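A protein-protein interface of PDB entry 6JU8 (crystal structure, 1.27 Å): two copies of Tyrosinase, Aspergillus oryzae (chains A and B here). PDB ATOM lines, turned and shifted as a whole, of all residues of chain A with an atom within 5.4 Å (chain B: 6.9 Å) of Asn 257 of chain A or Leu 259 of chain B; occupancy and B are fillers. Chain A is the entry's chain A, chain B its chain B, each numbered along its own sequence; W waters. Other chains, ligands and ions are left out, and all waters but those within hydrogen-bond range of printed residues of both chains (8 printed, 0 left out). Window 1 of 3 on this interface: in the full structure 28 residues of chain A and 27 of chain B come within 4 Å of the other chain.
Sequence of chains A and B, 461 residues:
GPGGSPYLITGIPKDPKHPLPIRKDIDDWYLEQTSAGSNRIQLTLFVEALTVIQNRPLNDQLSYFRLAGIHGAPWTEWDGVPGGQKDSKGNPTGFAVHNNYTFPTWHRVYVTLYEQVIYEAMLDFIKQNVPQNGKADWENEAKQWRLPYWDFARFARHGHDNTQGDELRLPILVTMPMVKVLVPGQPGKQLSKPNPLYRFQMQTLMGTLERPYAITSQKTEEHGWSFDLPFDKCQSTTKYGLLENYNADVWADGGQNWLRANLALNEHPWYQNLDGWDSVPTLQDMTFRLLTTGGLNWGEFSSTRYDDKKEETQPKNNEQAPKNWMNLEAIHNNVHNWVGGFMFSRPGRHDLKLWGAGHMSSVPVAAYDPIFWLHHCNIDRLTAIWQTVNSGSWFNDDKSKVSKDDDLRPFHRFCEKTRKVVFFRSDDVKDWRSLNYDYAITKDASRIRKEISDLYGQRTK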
ATOM      1  N   THR A 238     -13.585 -25.482 -10.331  1.00  0.00           N
ATOM      2  CA  THR A 238     -12.199 -25.915 -10.334  1.00  0.00           C
ATOM      3  C   THR A 238     -11.319 -24.903  -9.620  1.00  0.00           C
ATOM      4  O   THR A 238     -11.622 -23.708  -9.611  1.00  0.00           O
ATOM      5  CB  THR A 238     -11.712 -26.195 -11.759  1.00  0.00           C
ATOM      6  OG1 THR A 238     -10.352 -26.676 -11.759  1.00  0.00           O
ATOM      7  CG2 THR A 238     -11.740 -24.957 -12.652  1.00  0.00           C
ATOM      8  N   LYS A 239     -10.238 -25.388  -9.032  1.00  0.00           N
ATOM      9  CA  LYS A 239      -9.121 -24.559  -8.550  1.00  0.00           C
ATOM     10  C   LYS A 239      -7.957 -24.801  -9.496  1.00  0.00           C
ATOM     11  O   LYS A 239      -7.478 -25.961  -9.526  1.00  0.00           O
ATOM     12  CB  LYS A 239      -8.749 -24.890  -7.098  1.00  0.00           C
ATOM     13  CG  LYS A 239      -9.913 -24.765  -6.104  1.00  0.00           C
ATOM     14  CD  LYS A 239      -9.528 -25.501  -4.804  1.00  0.00           C
ATOM     15  CE  LYS A 239     -10.600 -25.363  -3.724  1.00  0.00           C
ATOM     16  NZ  LYS A 239     -11.911 -25.874  -4.202  1.00  0.00           N
ATOM     17  N   TYR A 240      -7.546 -23.829 -10.286  1.00  0.00           N
ATOM     18  CA  TYR A 240      -6.410 -23.852 -11.199  1.00  0.00           C
ATOM     19  C   TYR A 240      -6.592 -24.721 -12.438  1.00  0.00           C
ATOM     20  O   TYR A 240      -5.663 -24.777 -13.255  1.00  0.00           O
ATOM     21  CB  TYR A 240      -5.100 -24.278 -10.491  1.00  0.00           C
ATOM     22  CG  TYR A 240      -4.540 -23.207  -9.588  1.00  0.00           C
ATOM     23  CD1 TYR A 240      -5.050 -23.023  -8.302  1.00  0.00           C
ATOM     24  CD2 TYR A 240      -3.486 -22.368 -10.007  1.00  0.00           C
ATOM     25  CE1 TYR A 240      -4.554 -22.058  -7.442  1.00  0.00           C
ATOM     26  CE2 TYR A 240      -3.008 -21.388  -9.153  1.00  0.00           C
ATOM     27  CZ  TYR A 240      -3.537 -21.235  -7.879  1.00  0.00           C
ATOM     28  OH  TYR A 240      -3.015 -20.229  -7.081  1.00  0.00           O
ATOM     29  N   GLY A 241      -7.720 -25.405 -12.635  1.00  0.00           N
ATOM     30  CA  GLY A 241      -7.784 -26.366 -13.736  1.00  0.00           C
ATOM     31  C   GLY A 241      -8.074 -25.850 -15.127  1.00  0.00           C
ATOM     32  O   GLY A 241      -8.064 -26.684 -16.055  1.00  0.00           O
ATOM     33  N   LEU A 243      -6.757 -23.923 -18.257  1.00  0.00           N
ATOM     34  CA  LEU A 243      -5.535 -23.439 -18.890  1.00  0.00           C
ATOM     35  C   LEU A 243      -5.831 -23.176 -20.370  1.00  0.00           C
ATOM     36  O   LEU A 243      -6.514 -23.989 -21.011  1.00  0.00           O
ATOM     37  CB  LEU A 243      -4.393 -24.443 -18.754  1.00  0.00           C
ATOM     38  CG  LEU A 243      -3.659 -24.563 -17.415  1.00  0.00           C
ATOM     39  CD1 LEU A 243      -4.552 -25.019 -16.281  1.00  0.00           C
ATOM     40  CD2 LEU A 243      -2.468 -25.523 -17.581  1.00  0.00           C
ATOM     41  N   GLY A 254     -11.836 -29.453 -14.209  1.00  0.00           N
ATOM     42  CA  GLY A 254     -10.417 -29.230 -14.187  1.00  0.00           C
ATOM     43  C   GLY A 254      -9.725 -29.640 -12.913  1.00  0.00           C
ATOM     44  O   GLY A 254      -8.499 -29.540 -12.804  1.00  0.00           O
ATOM     45  N   GLY A 255     -10.494 -30.126 -11.940  1.00  0.00           N
ATOM     46  CA  GLY A 255      -9.966 -30.648 -10.707  1.00  0.00           C
ATOM     47  C   GLY A 255      -9.798 -29.634  -9.598  1.00  0.00           C
ATOM     48  O   GLY A 255      -9.886 -28.417  -9.772  1.00  0.00           O
ATOM     49  N   GLN A 256      -9.584 -30.157  -8.395  1.00  0.00           N
ATOM     50  CA  GLN A 256      -9.336 -29.360  -7.195  1.00  0.00           C
ATOM     51  C   GLN A 256      -7.830 -29.395  -6.973  1.00  0.00           C
ATOM     52  O   GLN A 256      -7.330 -30.282  -6.264  1.00  0.00           O
ATOM     53  CB  GLN A 256     -10.116 -29.946  -6.019  1.00  0.00           C
ATOM     54  CG  GLN A 256     -11.609 -30.114  -6.333  1.00  0.00           C
ATOM     55  CD  GLN A 256     -12.224 -28.897  -6.987  1.00  0.00           C
ATOM     56  OE1 GLN A 256     -12.035 -27.769  -6.533  1.00  0.00           O
ATOM     57  NE2 GLN A 256     -12.958 -29.112  -8.070  1.00  0.00           N
ATOM     58  N   ASN A 257      -7.117 -28.479  -7.628  1.00  0.00           N
ATOM     59  CA  ASN A 257      -5.648 -28.560  -7.625  1.00  0.00           C
ATOM     60  C   ASN A 257      -5.094 -27.835  -6.406  1.00  0.00           C
ATOM     61  O   ASN A 257      -4.467 -26.786  -6.466  1.00  0.00           O
ATOM     62  CB  ASN A 257      -5.116 -28.046  -8.954  1.00  0.00           C
ATOM     63  CG  ASN A 257      -5.695 -28.900 -10.083  1.00  0.00           C
ATOM     64  OD1 ASN A 257      -5.344 -30.073 -10.230  1.00  0.00           O
ATOM     65  ND2 ASN A 257      -6.611 -28.347 -10.869  1.00  0.00           N
ATOM     66  N   TRP A 258      -5.400 -28.416  -5.247  1.00  0.00           N
ATOM     67  CA  TRP A 258      -5.162 -27.822  -3.939  1.00  0.00           C
ATOM     68  C   TRP A 258      -3.691 -27.656  -3.609  1.00  0.00           C
ATOM     69  O   TRP A 258      -3.349 -26.750  -2.842  1.00  0.00           O
ATOM     70  CB  TRP A 258      -5.899 -28.607  -2.865  1.00  0.00           C
ATOM     71  CG  TRP A 258      -5.518 -30.041  -2.658  1.00  0.00           C
ATOM     72  CD1 TRP A 258      -6.103 -31.150  -3.213  1.00  0.00           C
ATOM     73  CD2 TRP A 258      -4.454 -30.524  -1.807  1.00  0.00           C
ATOM     74  NE1 TRP A 258      -5.474 -32.292  -2.768  1.00  0.00           N
ATOM     75  CE2 TRP A 258      -4.458 -31.928  -1.901  1.00  0.00           C
ATOM     76  CE3 TRP A 258      -3.520 -29.909  -0.973  1.00  0.00           C
ATOM     77  CZ2 TRP A 258      -3.548 -32.726  -1.198  1.00  0.00           C
ATOM     78  CZ3 TRP A 258      -2.611 -30.691  -0.272  1.00  0.00           C
ATOM     79  CH2 TRP A 258      -2.644 -32.105  -0.395  1.00  0.00           C
ATOM     80  N   LEU A 259      -2.793 -28.430  -4.217  1.00  0.00           N
ATOM     81  CA  LEU A 259      -1.368 -28.220  -3.938  1.00  0.00           C
ATOM     82  C   LEU A 259      -0.926 -26.890  -4.532  1.00  0.00           C
ATOM     83  O   LEU A 259      -0.035 -26.237  -3.973  1.00  0.00           O
ATOM     84  CB  LEU A 259      -0.514 -29.322  -4.582  1.00  0.00           C
ATOM     85  CG  LEU A 259      -0.684 -30.722  -3.982  1.00  0.00           C
ATOM     86  CD1 LEU A 259      -0.009 -31.737  -4.892  1.00  0.00           C
ATOM     87  CD2 LEU A 259      -0.092 -30.770  -2.579  1.00  0.00           C
ATOM     88  N   ARG A 260      -1.523 -26.507  -5.685  1.00  0.00           N
ATOM     89  CA  ARG A 260      -1.097 -25.251  -6.319  1.00  0.00           C
ATOM     90  C   ARG A 260      -1.641 -24.076  -5.512  1.00  0.00           C
ATOM     91  O   ARG A 260      -0.985 -23.055  -5.343  1.00  0.00           O
ATOM     92  CB  ARG A 260      -1.565 -25.210  -7.776  1.00  0.00           C
ATOM     93  CG  ARG A 260      -0.830 -24.123  -8.572  1.00  0.00           C
ATOM     94  CD  ARG A 260      -0.835 -24.491 -10.059  1.00  0.00           C
ATOM     95  NE  ARG A 260       0.179 -25.515 -10.292  1.00  0.00           N
ATOM     96  CZ  ARG A 260       0.815 -25.756 -11.416  1.00  0.00           C
ATOM     97  NH1 ARG A 260       0.517 -25.073 -12.512  1.00  0.00           N
ATOM     98  NH2 ARG A 260       1.761 -26.691 -11.456  1.00  0.00           N
ATOM     99  N   ALA A 261      -2.865 -24.217  -4.981  1.00  0.00           N
ATOM    100  CA  ALA A 261      -3.442 -23.184  -4.113  1.00  0.00           C
ATOM    101  C   ALA A 261      -2.573 -23.003  -2.868  1.00  0.00           C
ATOM    102  O   ALA A 261      -2.236 -21.899  -2.467  1.00  0.00           O
ATOM    103  CB  ALA A 261      -4.841 -23.571  -3.690  1.00  0.00           C
ATOM    104  N   TRP A 355       0.690 -21.576 -12.931  1.00  0.00           N
ATOM    105  CA  TRP A 355      -0.267 -21.483 -14.042  1.00  0.00           C
ATOM    106  C   TRP A 355      -1.576 -22.199 -13.727  1.00  0.00           C
ATOM    107  O   TRP A 355      -1.570 -23.303 -13.170  1.00  0.00           O
ATOM    108  CB  TRP A 355       0.372 -22.137 -15.268  1.00  0.00           C
ATOM    109  CG  TRP A 355      -0.362 -21.995 -16.566  1.00  0.00           C
ATOM    110  CD1 TRP A 355      -1.355 -21.119 -16.930  1.00  0.00           C
ATOM    111  CD2 TRP A 355      -0.109 -22.819 -17.716  1.00  0.00           C
ATOM    112  NE1 TRP A 355      -1.748 -21.335 -18.235  1.00  0.00           N
ATOM    113  CE2 TRP A 355      -0.984 -22.393 -18.736  1.00  0.00           C
ATOM    114  CE3 TRP A 355       0.771 -23.885 -17.959  1.00  0.00           C
ATOM    115  CZ2 TRP A 355      -1.006 -22.990 -19.992  1.00  0.00           C
ATOM    116  CZ3 TRP A 355       0.752 -24.480 -19.223  1.00  0.00           C
ATOM    117  CH2 TRP A 355      -0.124 -24.034 -20.228  1.00  0.00           C
ATOM    118  N   GLY A 356      -2.688 -21.562 -14.055  1.00  0.00           N
ATOM    119  CA  GLY A 356      -4.006 -22.133 -14.107  1.00  0.00           C
ATOM    120  C   GLY A 356      -5.055 -21.217 -13.519  1.00  0.00           C
ATOM    121  O   GLY A 356      -4.758 -20.444 -12.589  1.00  0.00           O
ATOM    122  N   GLU B 167       5.006 -27.827 -24.813  1.00  0.00           N
ATOM    123  CA  GLU B 167       4.787 -28.354 -23.470  1.00  0.00           C
ATOM    124  C   GLU B 167       4.533 -29.851 -23.560  1.00  0.00           C
ATOM    125  O   GLU B 167       3.708 -30.279 -24.368  1.00  0.00           O
ATOM    126  CB  GLU B 167       3.561 -27.689 -22.801  1.00  0.00           C
ATOM    127  CG  GLU B 167       3.384 -28.104 -21.351  1.00  0.00           C
ATOM    128  CD  GLU B 167       2.098 -27.743 -20.658  1.00  0.00           C
ATOM    129  OE1 GLU B 167       1.083 -27.366 -21.296  1.00  0.00           O
ATOM    130  OE2 GLU B 167       2.092 -27.869 -19.393  1.00  0.00           O
ATOM    131  N   LEU B 170       0.695 -34.865 -19.472  1.00  0.00           N
ATOM    132  CA  LEU B 170      -0.043 -36.123 -19.325  1.00  0.00           C
ATOM    133  C   LEU B 170      -1.140 -36.204 -20.381  1.00  0.00           C
ATOM    134  O   LEU B 170      -1.651 -35.152 -20.817  1.00  0.00           O
ATOM    135  CB  LEU B 170      -0.705 -36.181 -17.953  1.00  0.00           C
ATOM    136  CG  LEU B 170       0.197 -36.180 -16.722  1.00  0.00           C
ATOM    137  CD1 LEU B 170      -0.635 -36.486 -15.480  1.00  0.00           C
ATOM    138  CD2 LEU B 170       1.383 -37.101 -16.841  1.00  0.00           C
ATOM    139  N   THR B 175      -6.382 -36.962 -17.540  1.00  0.00           N
ATOM    140  CA  THR B 175      -6.640 -35.827 -16.648  1.00  0.00           C
ATOM    141  C   THR B 175      -8.130 -35.559 -16.476  1.00  0.00           C
ATOM    142  O   THR B 175      -8.484 -34.599 -15.794  1.00  0.00           O
ATOM    143  CB  THR B 175      -5.914 -34.559 -17.130  1.00  0.00           C
ATOM    144  OG1 THR B 175      -6.453 -34.052 -18.360  1.00  0.00           O
ATOM    145  CG2 THR B 175      -4.412 -34.800 -17.298  1.00  0.00           C
ATOM    146  N   TYR B 240       1.066 -37.058  -6.696  1.00  0.00           N
ATOM    147  CA  TYR B 240       1.548 -36.003  -5.833  1.00  0.00           C
ATOM    148  C   TYR B 240       0.744 -35.780  -4.566  1.00  0.00           C
ATOM    149  O   TYR B 240       1.105 -34.855  -3.806  1.00  0.00           O
ATOM    150  CB  TYR B 240       1.668 -34.648  -6.579  1.00  0.00           C
ATOM    151  CG  TYR B 240       2.835 -34.604  -7.542  1.00  0.00           C
ATOM    152  CD1 TYR B 240       2.743 -35.227  -8.783  1.00  0.00           C
ATOM    153  CD2 TYR B 240       4.041 -33.981  -7.193  1.00  0.00           C
ATOM    154  CE1 TYR B 240       3.816 -35.207  -9.676  1.00  0.00           C
ATOM    155  CE2 TYR B 240       5.094 -33.965  -8.086  1.00  0.00           C
ATOM    156  CZ  TYR B 240       4.983 -34.568  -9.315  1.00  0.00           C
ATOM    157  OH  TYR B 240       6.078 -34.550 -10.166  1.00  0.00           O
ATOM    158  N   GLN B 256      -5.558 -36.352  -8.375  1.00  0.00           N
ATOM    159  CA  GLN B 256      -4.737 -36.513  -9.586  1.00  0.00           C
ATOM    160  C   GLN B 256      -4.190 -35.132  -9.905  1.00  0.00           C
ATOM    161  O   GLN B 256      -4.843 -34.354 -10.611  1.00  0.00           O
ATOM    162  CB  GLN B 256      -5.562 -37.060 -10.757  1.00  0.00           C
ATOM    163  CG  GLN B 256      -6.389 -38.305 -10.413  1.00  0.00           C
ATOM    164  CD  GLN B 256      -5.535 -39.333  -9.690  1.00  0.00           C
ATOM    165  OE1 GLN B 256      -4.438 -39.662 -10.158  1.00  0.00           O
ATOM    166  NE2 GLN B 256      -6.046 -39.820  -8.577  1.00  0.00           N
ATOM    167  N   ASN B 257      -3.048 -34.817  -9.317  1.00  0.00           N
ATOM    168  CA  ASN B 257      -2.531 -33.441  -9.359  1.00  0.00           C
ATOM    169  C   ASN B 257      -1.704 -33.267 -10.629  1.00  0.00           C
ATOM    170  O   ASN B 257      -0.482 -33.124 -10.633  1.00  0.00           O
ATOM    171  CB  ASN B 257      -1.779 -33.128  -8.053  1.00  0.00           C
ATOM    172  CG  ASN B 257      -2.742 -33.300  -6.884  1.00  0.00           C
ATOM    173  OD1 ASN B 257      -3.644 -32.476  -6.750  1.00  0.00           O
ATOM    174  ND2 ASN B 257      -2.607 -34.345  -6.067  1.00  0.00           N
ATOM    175  N   TRP B 258      -2.438 -33.299 -11.742  1.00  0.00           N
ATOM    176  CA  TRP B 258      -1.825 -33.366 -13.064  1.00  0.00           C
ATOM    177  C   TRP B 258      -1.066 -32.115 -13.452  1.00  0.00           C
ATOM    178  O   TRP B 258      -0.163 -32.208 -14.289  1.00  0.00           O
ATOM    179  CB  TRP B 258      -2.867 -33.708 -14.120  1.00  0.00           C
ATOM    180  CG  TRP B 258      -4.047 -32.811 -14.258  1.00  0.00           C
ATOM    181  CD1 TRP B 258      -5.265 -32.900 -13.643  1.00  0.00           C
ATOM    182  CD2 TRP B 258      -4.127 -31.660 -15.124  1.00  0.00           C
ATOM    183  NE1 TRP B 258      -6.089 -31.882 -14.063  1.00  0.00           N
ATOM    184  CE2 TRP B 258      -5.413 -31.100 -14.969  1.00  0.00           C
ATOM    185  CE3 TRP B 258      -3.221 -31.053 -16.006  1.00  0.00           C
ATOM    186  CZ2 TRP B 258      -5.800 -29.956 -15.676  1.00  0.00           C
ATOM    187  CZ3 TRP B 258      -3.600 -29.922 -16.707  1.00  0.00           C
ATOM    188  CH2 TRP B 258      -4.890 -29.385 -16.526  1.00  0.00           C
ATOM    189  N   LEU B 259      -1.397 -30.950 -12.896  1.00  0.00           N
ATOM    190  CA  LEU B 259      -0.611 -29.757 -13.213  1.00  0.00           C
ATOM    191  C   LEU B 259       0.819 -29.904 -12.700  1.00  0.00           C
ATOM    192  O   LEU B 259       1.790 -29.421 -13.306  1.00  0.00           O
ATOM    193  CB  LEU B 259      -1.232 -28.509 -12.562  1.00  0.00           C
ATOM    194  CG  LEU B 259      -2.582 -28.073 -13.145  1.00  0.00           C
ATOM    195  CD1 LEU B 259      -3.215 -27.006 -12.283  1.00  0.00           C
ATOM    196  CD2 LEU B 259      -2.417 -27.503 -14.550  1.00  0.00           C
ATOM    197  N   ARG B 260       0.980 -30.554 -11.540  1.00  0.00           N
ATOM    198  CA  ARG B 260       2.302 -30.705 -10.943  1.00  0.00           C
ATOM    199  C   ARG B 260       3.110 -31.748 -11.692  1.00  0.00           C
ATOM    200  O   ARG B 260       4.325 -31.566 -11.929  1.00  0.00           O
ATOM    201  CB  ARG B 260       2.169 -31.038  -9.453  1.00  0.00           C
ATOM    202  CG  ARG B 260       3.487 -30.852  -8.711  1.00  0.00           C
ATOM    203  CD  ARG B 260       3.213 -30.662  -7.220  1.00  0.00           C
ATOM    204  NE  ARG B 260       2.699 -29.313  -6.991  1.00  0.00           N
ATOM    205  CZ  ARG B 260       2.757 -28.604  -5.884  1.00  0.00           C
ATOM    206  NH1 ARG B 260       3.253 -29.143  -4.777  1.00  0.00           N
ATOM    207  NH2 ARG B 260       2.265 -27.358  -5.866  1.00  0.00           N
ATOM    208  N   ALA B 261       2.456 -32.810 -12.141  1.00  0.00           N
ATOM    209  CA  ALA B 261       3.097 -33.769 -13.033  1.00  0.00           C
ATOM    210  C   ALA B 261       3.561 -33.092 -14.314  1.00  0.00           C
ATOM    211  O   ALA B 261       4.695 -33.291 -14.736  1.00  0.00           O
ATOM    212  CB  ALA B 261       2.143 -34.925 -13.329  1.00  0.00           C
ATOM    213  N   ASN B 262       2.703 -32.292 -14.952  1.00  0.00           N
ATOM    214  CA  ASN B 262       3.113 -31.574 -16.157  1.00  0.00           C
ATOM    215  C   ASN B 262       4.306 -30.678 -15.854  1.00  0.00           C
ATOM    216  O   ASN B 262       5.248 -30.604 -16.653  1.00  0.00           O
ATOM    217  CB  ASN B 262       1.968 -30.766 -16.777  1.00  0.00           C
ATOM    218  CG  ASN B 262       0.943 -31.656 -17.447  1.00  0.00           C
ATOM    219  OD1 ASN B 262       1.089 -32.890 -17.519  1.00  0.00           O
ATOM    220  ND2 ASN B 262      -0.113 -31.018 -17.963  1.00  0.00           N
ATOM    221  N   LEU B 263       4.287 -29.959 -14.741  1.00  0.00           N
ATOM    222  CA  LEU B 263       5.409 -29.076 -14.402  1.00  0.00           C
ATOM    223  C   LEU B 263       6.689 -29.890 -14.298  1.00  0.00           C
ATOM    224  O   LEU B 263       7.724 -29.489 -14.823  1.00  0.00           O
ATOM    225  CB  LEU B 263       5.124 -28.391 -13.062  1.00  0.00           C
ATOM    226  CG  LEU B 263       6.192 -27.377 -12.617  1.00  0.00           C
ATOM    227  CD1 LEU B 263       6.306 -26.230 -13.602  1.00  0.00           C
ATOM    228  CD2 LEU B 263       5.837 -26.906 -11.216  1.00  0.00           C
ATOM    229  N   ALA B 264       6.621 -31.043 -13.642  1.00  0.00           N
ATOM    230  CA  ALA B 264       7.803 -31.888 -13.484  1.00  0.00           C
ATOM    231  C   ALA B 264       8.333 -32.366 -14.832  1.00  0.00           C
ATOM    232  O   ALA B 264       9.550 -32.378 -15.062  1.00  0.00           O
ATOM    233  CB  ALA B 264       7.494 -33.083 -12.585  1.00  0.00           C
ATOM    234  N   LYS B 353       7.459 -26.144  -5.279  1.00  0.00           N
ATOM    235  CA  LYS B 353       6.588 -26.222  -6.449  1.00  0.00           C
ATOM    236  C   LYS B 353       6.358 -27.648  -6.924  1.00  0.00           C
ATOM    237  O   LYS B 353       5.412 -27.851  -7.693  1.00  0.00           O
ATOM    238  CB  LYS B 353       7.141 -25.403  -7.621  1.00  0.00           C
ATOM    239  CG  LYS B 353       8.554 -25.832  -8.005  1.00  0.00           C
ATOM    240  CD  LYS B 353       9.091 -24.944  -9.126  1.00  0.00           C
ATOM    241  CE  LYS B 353      10.510 -25.380  -9.490  1.00  0.00           C
ATOM    242  NZ  LYS B 353      11.001 -24.570 -10.647  1.00  0.00           N
ATOM    243  N   LEU B 354       7.182 -28.599  -6.512  1.00  0.00           N
ATOM    244  CA  LEU B 354       7.050 -29.985  -6.938  1.00  0.00           C
ATOM    245  C   LEU B 354       6.797 -30.924  -5.769  1.00  0.00           C
ATOM    246  O   LEU B 354       6.913 -32.145  -5.953  1.00  0.00           O
ATOM    247  CB  LEU B 354       8.287 -30.441  -7.720  1.00  0.00           C
ATOM    248  CG  LEU B 354       8.379 -29.931  -9.173  1.00  0.00           C
ATOM    249  CD1 LEU B 354       9.625 -30.527  -9.828  1.00  0.00           C
ATOM    250  CD2 LEU B 354       7.159 -30.266 -10.003  1.00  0.00           C
HETATM  251  O   HOH W   1      -2.627 -30.557 -10.279  1.00  0.00           O
HETATM  252  O   HOH W   2      -6.794 -32.311 -10.400  1.00  0.00           O
HETATM  253  O   HOH W   3      -9.105 -32.492 -14.235  1.00  0.00           O
HETATM  254  O   HOH W   4       3.134 -26.300  -8.708  1.00  0.00           O
HETATM  255  O   HOH W   5       1.287 -27.162 -14.821  1.00  0.00           O
HETATM  256  O   HOH W   6      -6.304 -32.860  -6.384  1.00  0.00           O
HETATM  257  O   HOH W   7      -3.024 -29.837  -6.779  1.00  0.00           O
HETATM  258  O   HOH W   8       1.888 -27.495  -2.484  1.00  0.00           O
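ND2 of Asn 257 of chain A sits at hydrogen-bond distance from O of Gly 255 of chain A. The backbone carbonyl oxygen (O) of Gly 254 of chain A sits at hydrogen-bond distance from the side-chain amide nitrogen (ND2) of Asn 257 of chain A (3.0 Å). The guanidinium group of Arg 260 of chain B is in hydrogen-bond range of the backbone carbonyl oxygen of Lys 353 of chain B (3.2 Å). The guanidinium group (NH1) of Arg 260 of chain A lies within hydrogen-bond range of the backbone carbonyl oxygen (O) of Trp 355 of chain A (2.8 Å). OG1 of Thr 238 of chain A sits at hydrogen-bond distance from N of Gly 241 of chain A (3.1 Å). O of Lys 239 of chain A sits at hydrogen-bond distance from ND2 of Asn 257 of chain A, 2.9 Å away.
Tyr 240 of chain A touches Leu 259 of chain B, and with the chains exchanged Leu 259 of chain A touches Tyr 240 of chain B. Asn 257 of chain A touches Leu 259 of chain B, and with the chains exchanged Leu 259 of chain A touches Asn 257 of chain B. Leu 259 of chain A touches Arg 260 of chain B, and with the chains exchanged Arg 260 of chain A touches Leu 259 of chain B. Arg 260 of chain B touches its own counterpart, Arg 260 of chain A. Positions printed for both chains: 240, 256, 257, 258, 259, 260 and 261.
Of the 15 printed residues of chain A, 8 touch a printed residue of chain B. Hydrophobic or aromatic side chains of chain A that line the printed part of chain B: Tyr 240, Leu 243, Leu 259 and Trp 355.
Water W3 lies within hydrogen-bond range of the backbone carbonyl oxygen (O) of Thr 175 of chain B, the indole nitrogen (NE1) of Trp 258 of chain B and the backbone carbonyl oxygen (O) of Gly 254 of chain A. Water W7 lies within hydrogen-bond range of OD1 of Asn 257 of chain B, N of Leu 259 of chain A, N of Trp 258 of chain A and O of Asn 257 of chain A. Water W6 bridges the side-chain amide oxygen (OD1) of Asn 257 of chain B (2.7 Å) and the backbone carbonyl oxygen (O) of Gln 256 of chain A (2.8 Å). Water W8 lies within hydrogen-bond range of the backbone carbonyl oxygen of Leu 259 of chain A (2.7 Å) and the guanidinium group of Arg 260 of chain B (3.1 Å). Water W1 lies within hydrogen-bond range of OD1 of Asn 257 of chain A (2.8 Å), N of Leu 259 of chain B (2.9 Å), N of Trp 258 of chain B (3.1 Å) and O of Asn 257 of chain B (3.4 Å). Water W5 lies within hydrogen-bond range of O of Leu 259 of chain B (2.8 Å) and NH1 of Arg 260 of chain A (3.2 Å).
O of Tyr 240 of chain A touches CD1 of Leu 259 of chain B, at 3.5 Å. Trp 258 of chain B touches Gly 241 of chain A (CZ2 to O, 3.997 Å). Leu 259 of chain B touches Leu 243 of chain A (CD2 to CD2, 3.6 Å). NE1 of Trp 258 of chain B touches O of Gly 254 of chain A, 3.6 Å away. Asn 257 of chain A touches Leu 259 of chain B. Leu 259 of chain A touches Tyr 240 of chain B. Leu 259 of chain A touches Asn 257 of chain B. Arg 260 of chain A touches Arg 260 of chain B (N to NH2, 3.9 Å). OE1 of Glu 167 of chain B touches CZ3 of Trp 355 of chain A (3.6 Å).
Thr 238 of chain A touches none of the printed residues of chain B. Of the printed residues of chain B, Tyr 240 of chain A touches Leu 259. Of the printed residues of chain B, Leu 243 of chain A touches Leu 259. Asn 257 of chain A touches one residue of chain B. Printed residues of chain B within 4 Å of Trp 355 of chain A: Glu 167. Printed residues of chain A within 4 Å of Glu 167 of chain B: Trp 355 (3.6 Å). Of the printed residues of chain A, Tyr 240 of chain B touches Leu 259 (3.5 Å). Of chain A, only Tyr 240, Leu 243, Asn 257 and Arg 260 come within 4 Å of Leu 259 of chain B. The nearest printed residue of chain B that does not touch Asn 257 of chain A is Trp 258 of chain B (4.3 Å). The nearest residue of chain A that does not touch Leu 259 of chain B is Trp 355 of chain A (4.1 Å).
The backbone carbonyl oxygen (O) of Leu 259 of chain A is in hydrogen-bond range of the guanidinium group (NH2) of Arg 260 of chain B, at 3.2 Å. The backbone carbonyl oxygen (O) of Leu 259 of chain B is in hydrogen-bond range of the guanidinium group (NH2) of Arg 260 of chain A (3.3 Å).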
